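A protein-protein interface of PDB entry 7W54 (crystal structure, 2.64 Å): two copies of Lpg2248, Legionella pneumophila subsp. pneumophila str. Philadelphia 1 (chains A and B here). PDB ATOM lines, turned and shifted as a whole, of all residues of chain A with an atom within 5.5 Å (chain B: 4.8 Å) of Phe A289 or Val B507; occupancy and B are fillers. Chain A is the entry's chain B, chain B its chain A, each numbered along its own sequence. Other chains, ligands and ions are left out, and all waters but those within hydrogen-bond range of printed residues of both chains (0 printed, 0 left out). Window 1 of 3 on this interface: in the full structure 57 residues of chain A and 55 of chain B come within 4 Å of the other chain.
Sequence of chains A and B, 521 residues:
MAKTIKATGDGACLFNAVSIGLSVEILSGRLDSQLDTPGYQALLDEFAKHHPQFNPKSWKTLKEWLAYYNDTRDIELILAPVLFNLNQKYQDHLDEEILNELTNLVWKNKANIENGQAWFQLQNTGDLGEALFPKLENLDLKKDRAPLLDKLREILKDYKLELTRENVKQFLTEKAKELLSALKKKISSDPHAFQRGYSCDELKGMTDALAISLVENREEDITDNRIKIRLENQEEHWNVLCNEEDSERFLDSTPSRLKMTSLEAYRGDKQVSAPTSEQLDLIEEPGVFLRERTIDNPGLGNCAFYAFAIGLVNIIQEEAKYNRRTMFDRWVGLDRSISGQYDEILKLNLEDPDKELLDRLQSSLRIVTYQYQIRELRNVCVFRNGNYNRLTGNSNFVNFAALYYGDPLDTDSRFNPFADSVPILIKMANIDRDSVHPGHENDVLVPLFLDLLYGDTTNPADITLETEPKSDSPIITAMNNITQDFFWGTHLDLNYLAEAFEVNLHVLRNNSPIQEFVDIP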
ATOM      1  N   ILE A 283      28.714 -11.193  22.100  1.00  0.00           N
ATOM      2  CA  ILE A 283      29.438 -11.696  23.265  1.00  0.00           C
ATOM      3  C   ILE A 283      28.511 -11.791  24.466  1.00  0.00           C
ATOM      4  O   ILE A 283      28.548 -12.760  25.238  1.00  0.00           O
ATOM      5  CB  ILE A 283      30.641 -10.777  23.565  1.00  0.00           C
ATOM      6  CG1 ILE A 283      31.345 -11.202  24.830  1.00  0.00           C
ATOM      7  CG2 ILE A 283      30.209  -9.374  23.815  1.00  0.00           C
ATOM      8  CD1 ILE A 283      31.871 -12.526  24.739  1.00  0.00           C
ATOM      9  N   GLY A 287      22.553 -16.011  27.733  1.00  0.00           N
ATOM     10  CA  GLY A 287      22.894 -17.391  27.447  1.00  0.00           C
ATOM     11  C   GLY A 287      22.561 -18.302  28.608  1.00  0.00           C
ATOM     12  O   GLY A 287      22.656 -17.920  29.776  1.00  0.00           O
ATOM     13  N   VAL A 288      22.157 -19.521  28.266  1.00  0.00           N
ATOM     14  CA  VAL A 288      21.949 -20.596  29.226  1.00  0.00           C
ATOM     15  C   VAL A 288      23.037 -21.633  29.001  1.00  0.00           C
ATOM     16  O   VAL A 288      23.205 -22.130  27.880  1.00  0.00           O
ATOM     17  CB  VAL A 288      20.551 -21.222  29.088  1.00  0.00           C
ATOM     18  CG1 VAL A 288      20.454 -22.487  29.925  1.00  0.00           C
ATOM     19  CG2 VAL A 288      19.481 -20.224  29.493  1.00  0.00           C
ATOM     20  N   PHE A 289      23.776 -21.954  30.055  1.00  0.00           N
ATOM     21  CA  PHE A 289      24.909 -22.866  29.971  1.00  0.00           C
ATOM     22  C   PHE A 289      24.576 -24.135  30.742  1.00  0.00           C
ATOM     23  O   PHE A 289      24.399 -24.098  31.964  1.00  0.00           O
ATOM     24  CB  PHE A 289      26.174 -22.199  30.507  1.00  0.00           C
ATOM     25  CG  PHE A 289      26.547 -20.947  29.765  1.00  0.00           C
ATOM     26  CD1 PHE A 289      27.355 -21.004  28.643  1.00  0.00           C
ATOM     27  CD2 PHE A 289      26.068 -19.715  30.176  1.00  0.00           C
ATOM     28  CE1 PHE A 289      27.691 -19.854  27.951  1.00  0.00           C
ATOM     29  CE2 PHE A 289      26.400 -18.562  29.488  1.00  0.00           C
ATOM     30  CZ  PHE A 289      27.213 -18.632  28.373  1.00  0.00           C
ATOM     31  N   LEU A 290      24.490 -25.251  30.024  1.00  0.00           N
ATOM     32  CA  LEU A 290      24.089 -26.529  30.588  1.00  0.00           C
ATOM     33  C   LEU A 290      25.205 -27.552  30.430  1.00  0.00           C
ATOM     34  O   LEU A 290      26.140 -27.372  29.646  1.00  0.00           O
ATOM     35  CB  LEU A 290      22.812 -27.052  29.923  1.00  0.00           C
ATOM     36  CG  LEU A 290      21.620 -26.101  29.968  1.00  0.00           C
ATOM     37  CD1 LEU A 290      20.411 -26.768  29.360  1.00  0.00           C
ATOM     38  CD2 LEU A 290      21.339 -25.681  31.398  1.00  0.00           C
ATOM     39  N   ARG A 291      25.085 -28.643  31.182  1.00  0.00           N
ATOM     40  CA  ARG A 291      26.064 -29.720  31.166  1.00  0.00           C
ATOM     41  C   ARG A 291      25.327 -31.048  31.105  1.00  0.00           C
ATOM     42  O   ARG A 291      24.590 -31.393  32.033  1.00  0.00           O
ATOM     43  CB  ARG A 291      26.967 -29.665  32.400  1.00  0.00           C
ATOM     44  CG  ARG A 291      27.923 -30.838  32.522  1.00  0.00           C
ATOM     45  CD  ARG A 291      29.106 -30.482  33.397  1.00  0.00           C
ATOM     46  NE  ARG A 291      30.323 -30.289  32.616  1.00  0.00           N
ATOM     47  CZ  ARG A 291      31.276 -29.417  32.923  1.00  0.00           C
ATOM     48  NH1 ARG A 291      31.151 -28.647  33.997  1.00  0.00           N
ATOM     49  NH2 ARG A 291      32.352 -29.312  32.157  1.00  0.00           N
ATOM     50  N   ASN A 504      20.729 -17.872  24.090  1.00  0.00           N
ATOM     51  CA  ASN A 504      21.693 -18.761  23.456  1.00  0.00           C
ATOM     52  C   ASN A 504      21.946 -19.953  24.369  1.00  0.00           C
ATOM     53  O   ASN A 504      22.428 -19.790  25.495  1.00  0.00           O
ATOM     54  CB  ASN A 504      23.001 -18.038  23.145  1.00  0.00           C
ATOM     55  CG  ASN A 504      23.799 -18.730  22.053  1.00  0.00           C
ATOM     56  OD1 ASN A 504      24.980 -19.027  22.223  1.00  0.00           O
ATOM     57  ND2 ASN A 504      23.150 -18.995  20.924  1.00  0.00           N
ATOM     58  N   LEU A 505      21.617 -21.145  23.886  1.00  0.00           N
ATOM     59  CA  LEU A 505      21.814 -22.369  24.646  1.00  0.00           C
ATOM     60  C   LEU A 505      23.199 -22.934  24.361  1.00  0.00           C
ATOM     61  O   LEU A 505      23.560 -23.158  23.202  1.00  0.00           O
ATOM     62  CB  LEU A 505      20.740 -23.397  24.295  1.00  0.00           C
ATOM     63  CG  LEU A 505      20.870 -24.767  24.954  1.00  0.00           C
ATOM     64  CD1 LEU A 505      20.722 -24.634  26.458  1.00  0.00           C
ATOM     65  CD2 LEU A 505      19.831 -25.717  24.392  1.00  0.00           C
ATOM     66  N   HIS A 506      23.976 -23.143  25.421  1.00  0.00           N
ATOM     67  CA  HIS A 506      25.282 -23.781  25.340  1.00  0.00           C
ATOM     68  C   HIS A 506      25.231 -25.070  26.144  1.00  0.00           C
ATOM     69  O   HIS A 506      24.766 -25.073  27.288  1.00  0.00           O
ATOM     70  CB  HIS A 506      26.391 -22.875  25.878  1.00  0.00           C
ATOM     71  CG  HIS A 506      26.365 -21.482  25.327  1.00  0.00           C
ATOM     72  ND1 HIS A 506      27.344 -20.997  24.488  1.00  0.00           N
ATOM     73  CD2 HIS A 506      25.489 -20.466  25.508  1.00  0.00           C
ATOM     74  CE1 HIS A 506      27.070 -19.745  24.169  1.00  0.00           C
ATOM     75  NE2 HIS A 506      25.947 -19.400  24.773  1.00  0.00           N
ATOM     76  N   PHE A 517      40.490 -17.007  30.606  1.00  0.00           N
ATOM     77  CA  PHE A 517      41.350 -16.055  29.920  1.00  0.00           C
ATOM     78  C   PHE A 517      40.848 -14.647  30.201  1.00  0.00           C
ATOM     79  O   PHE A 517      39.673 -14.437  30.511  1.00  0.00           O
ATOM     80  CB  PHE A 517      41.407 -16.325  28.410  1.00  0.00           C
ATOM     81  CG  PHE A 517      40.215 -15.814  27.653  1.00  0.00           C
ATOM     82  CD1 PHE A 517      39.021 -16.517  27.654  1.00  0.00           C
ATOM     83  CD2 PHE A 517      40.293 -14.636  26.923  1.00  0.00           C
ATOM     84  CE1 PHE A 517      37.927 -16.052  26.951  1.00  0.00           C
ATOM     85  CE2 PHE A 517      39.203 -14.166  26.218  1.00  0.00           C
ATOM     86  CZ  PHE A 517      38.018 -14.874  26.232  1.00  0.00           C
ATOM     87  N   LEU B 290      35.427 -21.464  26.857  1.00  0.00           N
ATOM     88  CA  LEU B 290      36.229 -20.524  27.619  1.00  0.00           C
ATOM     89  C   LEU B 290      35.331 -19.746  28.567  1.00  0.00           C
ATOM     90  O   LEU B 290      34.114 -19.692  28.390  1.00  0.00           O
ATOM     91  CB  LEU B 290      36.970 -19.548  26.694  1.00  0.00           C
ATOM     92  CG  LEU B 290      37.629 -20.169  25.467  1.00  0.00           C
ATOM     93  CD1 LEU B 290      38.162 -19.083  24.552  1.00  0.00           C
ATOM     94  CD2 LEU B 290      38.739 -21.113  25.886  1.00  0.00           C
ATOM     95  N   LEU B 505      32.765 -21.904  19.373  1.00  0.00           N
ATOM     96  CA  LEU B 505      33.379 -21.205  20.490  1.00  0.00           C
ATOM     97  C   LEU B 505      32.283 -20.706  21.427  1.00  0.00           C
ATOM     98  O   LEU B 505      31.406 -19.938  21.015  1.00  0.00           O
ATOM     99  CB  LEU B 505      34.242 -20.046  20.001  1.00  0.00           C
ATOM    100  CG  LEU B 505      34.894 -19.230  21.115  1.00  0.00           C
ATOM    101  CD1 LEU B 505      35.841 -20.105  21.919  1.00  0.00           C
ATOM    102  CD2 LEU B 505      35.618 -18.028  20.552  1.00  0.00           C
ATOM    103  N   HIS B 506      32.340 -21.160  22.681  1.00  0.00           N
ATOM    104  CA  HIS B 506      31.424 -20.766  23.742  1.00  0.00           C
ATOM    105  C   HIS B 506      32.222 -20.049  24.817  1.00  0.00           C
ATOM    106  O   HIS B 506      33.100 -20.651  25.444  1.00  0.00           O
ATOM    107  CB  HIS B 506      30.722 -21.987  24.352  1.00  0.00           C
ATOM    108  CG  HIS B 506      30.135 -22.937  23.355  1.00  0.00           C
ATOM    109  ND1 HIS B 506      28.793 -22.948  23.042  1.00  0.00           N
ATOM    110  CD2 HIS B 506      30.700 -23.929  22.629  1.00  0.00           C
ATOM    111  CE1 HIS B 506      28.557 -23.902  22.161  1.00  0.00           C
ATOM    112  NE2 HIS B 506      29.698 -24.513  21.894  1.00  0.00           N
ATOM    113  N   VAL B 507      31.927 -18.780  25.036  1.00  0.00           N
ATOM    114  CA  VAL B 507      32.595 -18.030  26.087  1.00  0.00           C
ATOM    115  C   VAL B 507      31.542 -17.686  27.141  1.00  0.00           C
ATOM    116  O   VAL B 507      30.530 -17.038  26.839  1.00  0.00           O
ATOM    117  CB  VAL B 507      33.348 -16.810  25.504  1.00  0.00           C
ATOM    118  CG1 VAL B 507      34.162 -17.217  24.269  1.00  0.00           C
ATOM    119  CG2 VAL B 507      32.447 -15.694  25.111  1.00  0.00           C
ATOM    120  N   LEU B 508      31.701 -18.249  28.344  1.00  0.00           N
ATOM    121  CA  LEU B 508      30.959 -17.916  29.547  1.00  0.00           C
ATOM    122  C   LEU B 508      31.458 -16.577  30.055  1.00  0.00           C
ATOM    123  O   LEU B 508      32.564 -16.141  29.718  1.00  0.00           O
ATOM    124  CB  LEU B 508      31.154 -18.996  30.603  1.00  0.00           C
ATOM    125  CG  LEU B 508      30.432 -20.338  30.449  1.00  0.00           C
ATOM    126  CD1 LEU B 508      30.814 -21.080  29.157  1.00  0.00           C
ATOM    127  CD2 LEU B 508      30.773 -21.203  31.622  1.00  0.00           C
ATOM    128  N   ARG B 509      30.630 -15.914  30.842  1.00  0.00           N
ATOM    129  CA  ARG B 509      31.087 -14.740  31.557  1.00  0.00           C
ATOM    130  C   ARG B 509      31.732 -15.167  32.872  1.00  0.00           C
ATOM    131  O   ARG B 509      31.706 -16.340  33.253  1.00  0.00           O
ATOM    132  CB  ARG B 509      29.931 -13.774  31.798  1.00  0.00           C
ATOM    133  CG  ARG B 509      29.131 -13.473  30.553  1.00  0.00           C
ATOM    134  CD  ARG B 509      28.931 -11.989  30.367  1.00  0.00           C
ATOM    135  NE  ARG B 509      30.032 -11.375  29.630  1.00  0.00           N
ATOM    136  CZ  ARG B 509      29.929 -10.233  28.960  1.00  0.00           C
ATOM    137  NH1 ARG B 509      28.776  -9.581  28.936  1.00  0.00           N
ATOM    138  NH2 ARG B 509      30.980  -9.740  28.317  1.00  0.00           N
ATOM    139  N   SER B 512      28.878 -16.821  34.922  1.00  0.00           N
ATOM    140  CA  SER B 512      27.847 -17.638  34.291  1.00  0.00           C
ATOM    141  C   SER B 512      27.662 -18.935  35.070  1.00  0.00           C
ATOM    142  O   SER B 512      28.645 -19.625  35.357  1.00  0.00           O
ATOM    143  CB  SER B 512      28.210 -17.952  32.841  1.00  0.00           C
ATOM    144  OG  SER B 512      28.534 -16.774  32.122  1.00  0.00           O
ATOM    145  N   PRO B 513      26.435 -19.292  35.437  1.00  0.00           N
ATOM    146  CA  PRO B 513      26.194 -20.572  36.105  1.00  0.00           C
ATOM    147  C   PRO B 513      25.964 -21.699  35.107  1.00  0.00           C
ATOM    148  O   PRO B 513      25.537 -21.488  33.969  1.00  0.00           O
ATOM    149  CB  PRO B 513      24.923 -20.296  36.918  1.00  0.00           C
ATOM    150  CG  PRO B 513      24.176 -19.323  36.068  1.00  0.00           C
ATOM    151  CD  PRO B 513      25.210 -18.477  35.351  1.00  0.00           C
ATOM    152  N   ILE B 514      26.255 -22.915  35.561  1.00  0.00           N
ATOM    153  CA  ILE B 514      26.149 -24.114  34.737  1.00  0.00           C
ATOM    154  C   ILE B 514      25.264 -25.112  35.469  1.00  0.00           C
ATOM    155  O   ILE B 514      25.641 -25.617  36.533  1.00  0.00           O
ATOM    156  CB  ILE B 514      27.518 -24.730  34.426  1.00  0.00           C
ATOM    157  CG1 ILE B 514      28.437 -23.693  33.779  1.00  0.00           C
ATOM    158  CG2 ILE B 514      27.359 -25.941  33.517  1.00  0.00           C
ATOM    159  CD1 ILE B 514      29.871 -24.151  33.639  1.00  0.00           C
ATOM    160  N   GLN B 515      24.098 -25.400  34.902  1.00  0.00           N
ATOM    161  CA  GLN B 515      23.178 -26.391  35.441  1.00  0.00           C
ATOM    162  C   GLN B 515      23.288 -27.671  34.627  1.00  0.00           C
ATOM    163  O   GLN B 515      23.325 -27.629  33.395  1.00  0.00           O
ATOM    164  CB  GLN B 515      21.735 -25.884  35.402  1.00  0.00           C
ATOM    165  CG  GLN B 515      21.512 -24.579  36.131  1.00  0.00           C
ATOM    166  CD  GLN B 515      21.982 -23.374  35.342  1.00  0.00           C
ATOM    167  OE1 GLN B 515      22.723 -22.537  35.853  1.00  0.00           O
ATOM    168  NE2 GLN B 515      21.561 -23.286  34.086  1.00  0.00           N
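N of Arg A291 sits at hydrogen-bond distance from O of Gln B515 (3.0 Å).
N of Gln B515 is in hydrogen-bond range of O of Phe A289, at 3.2 Å.
The backbone carbonyl oxygen (O) of Pro B513 lies close to the backbone carbonyl oxygen (O) of Phe A289 (3.5 Å).
ND1 of His A506 is in hydrogen-bond range of ND1 of His B506, at 2.8 Å.
The backbone carbonyl oxygen of Val A288 sits at hydrogen-bond distance from the backbone NH of His A506 (2.8 Å).
The backbone NH (N) of Leu A290 is in hydrogen-bond range of the backbone carbonyl oxygen (O) of His A506 (2.8 Å).
O of Leu B290 lies within hydrogen-bond range of N of Leu B508.
The side-chain amide oxygen of Asn A504 lies within hydrogen-bond range of a ring nitrogen (NE2) of His A506.
The backbone NH (N) of Leu B290 lies within hydrogen-bond range of the backbone carbonyl oxygen (O) of His B506.
The backbone NH of Arg B509 lies within hydrogen-bond range of the side-chain hydroxyl of Ser B512 (2.6 Å).
Among the printed residues, pairs that only touch across the chains: Ile A283 with Val B507 (3.2 Å), Ile A283 with Arg B509 (3.8 Å), Phe A289 with Val B507 (3.99 Å), Phe A289 with Leu B508 (3.5 Å), Phe A289 with Ser B512 (3.8 Å), Phe A289 with Ile B514 (3.3 Å), Leu A290 with Gln B515 (3.1 Å), Arg A291 with Ile B514 (3.9 Å) and Phe A517 with Leu B290 (3.6 Å).
Of the printed residues of chain B, Phe A289 touches Val B507 (3.99 Å), Leu B508 (3.5 Å), Ser B512 (3.8 Å), Pro B513 (3.5 Å), Ile B514 (3.3 Å) and Gln B515 (3.2 Å).
Of the printed residues of chain A, Val B507 touches Ile A283 and Phe A289.
Of the printed residues of chain B, Leu A290 touches Gln B515.
Of the printed residues of chain A, Ser B512 touches Phe A289.
Of the printed residues of chain B, Arg A291 touches Ile B514 (3.9 Å) and Gln B515 (3.0 Å).
Of the printed residues of chain B, Phe A517 touches Leu B290.
Leu A505 touches none of the printed residues of chain B.
Asn A504 touches none of the printed residues of chain B.
Along chain B the printed residues that touch a printed residue of chain A span positions 290 to 515.
Of the 10 printed residues of chain A, 6 touch a printed residue of chain B.
Hydrophobic or aromatic side chains of chain A that line the printed part of chain B: Ile A283, Phe A289, Leu A290, His A506 and Phe A517.
Among the printed residues, 13 pairs touch across the chains.
Among the printed residues, no Asp or Glu carboxylate lies within 4 Å of a Lys or Arg side-chain nitrogen of the other chain.
His A506 touches its own counterpart, His B506.
Of the 13 pairs that touch across the chains among the printed residues, 1 has its exchanged pair printed and touching as well.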
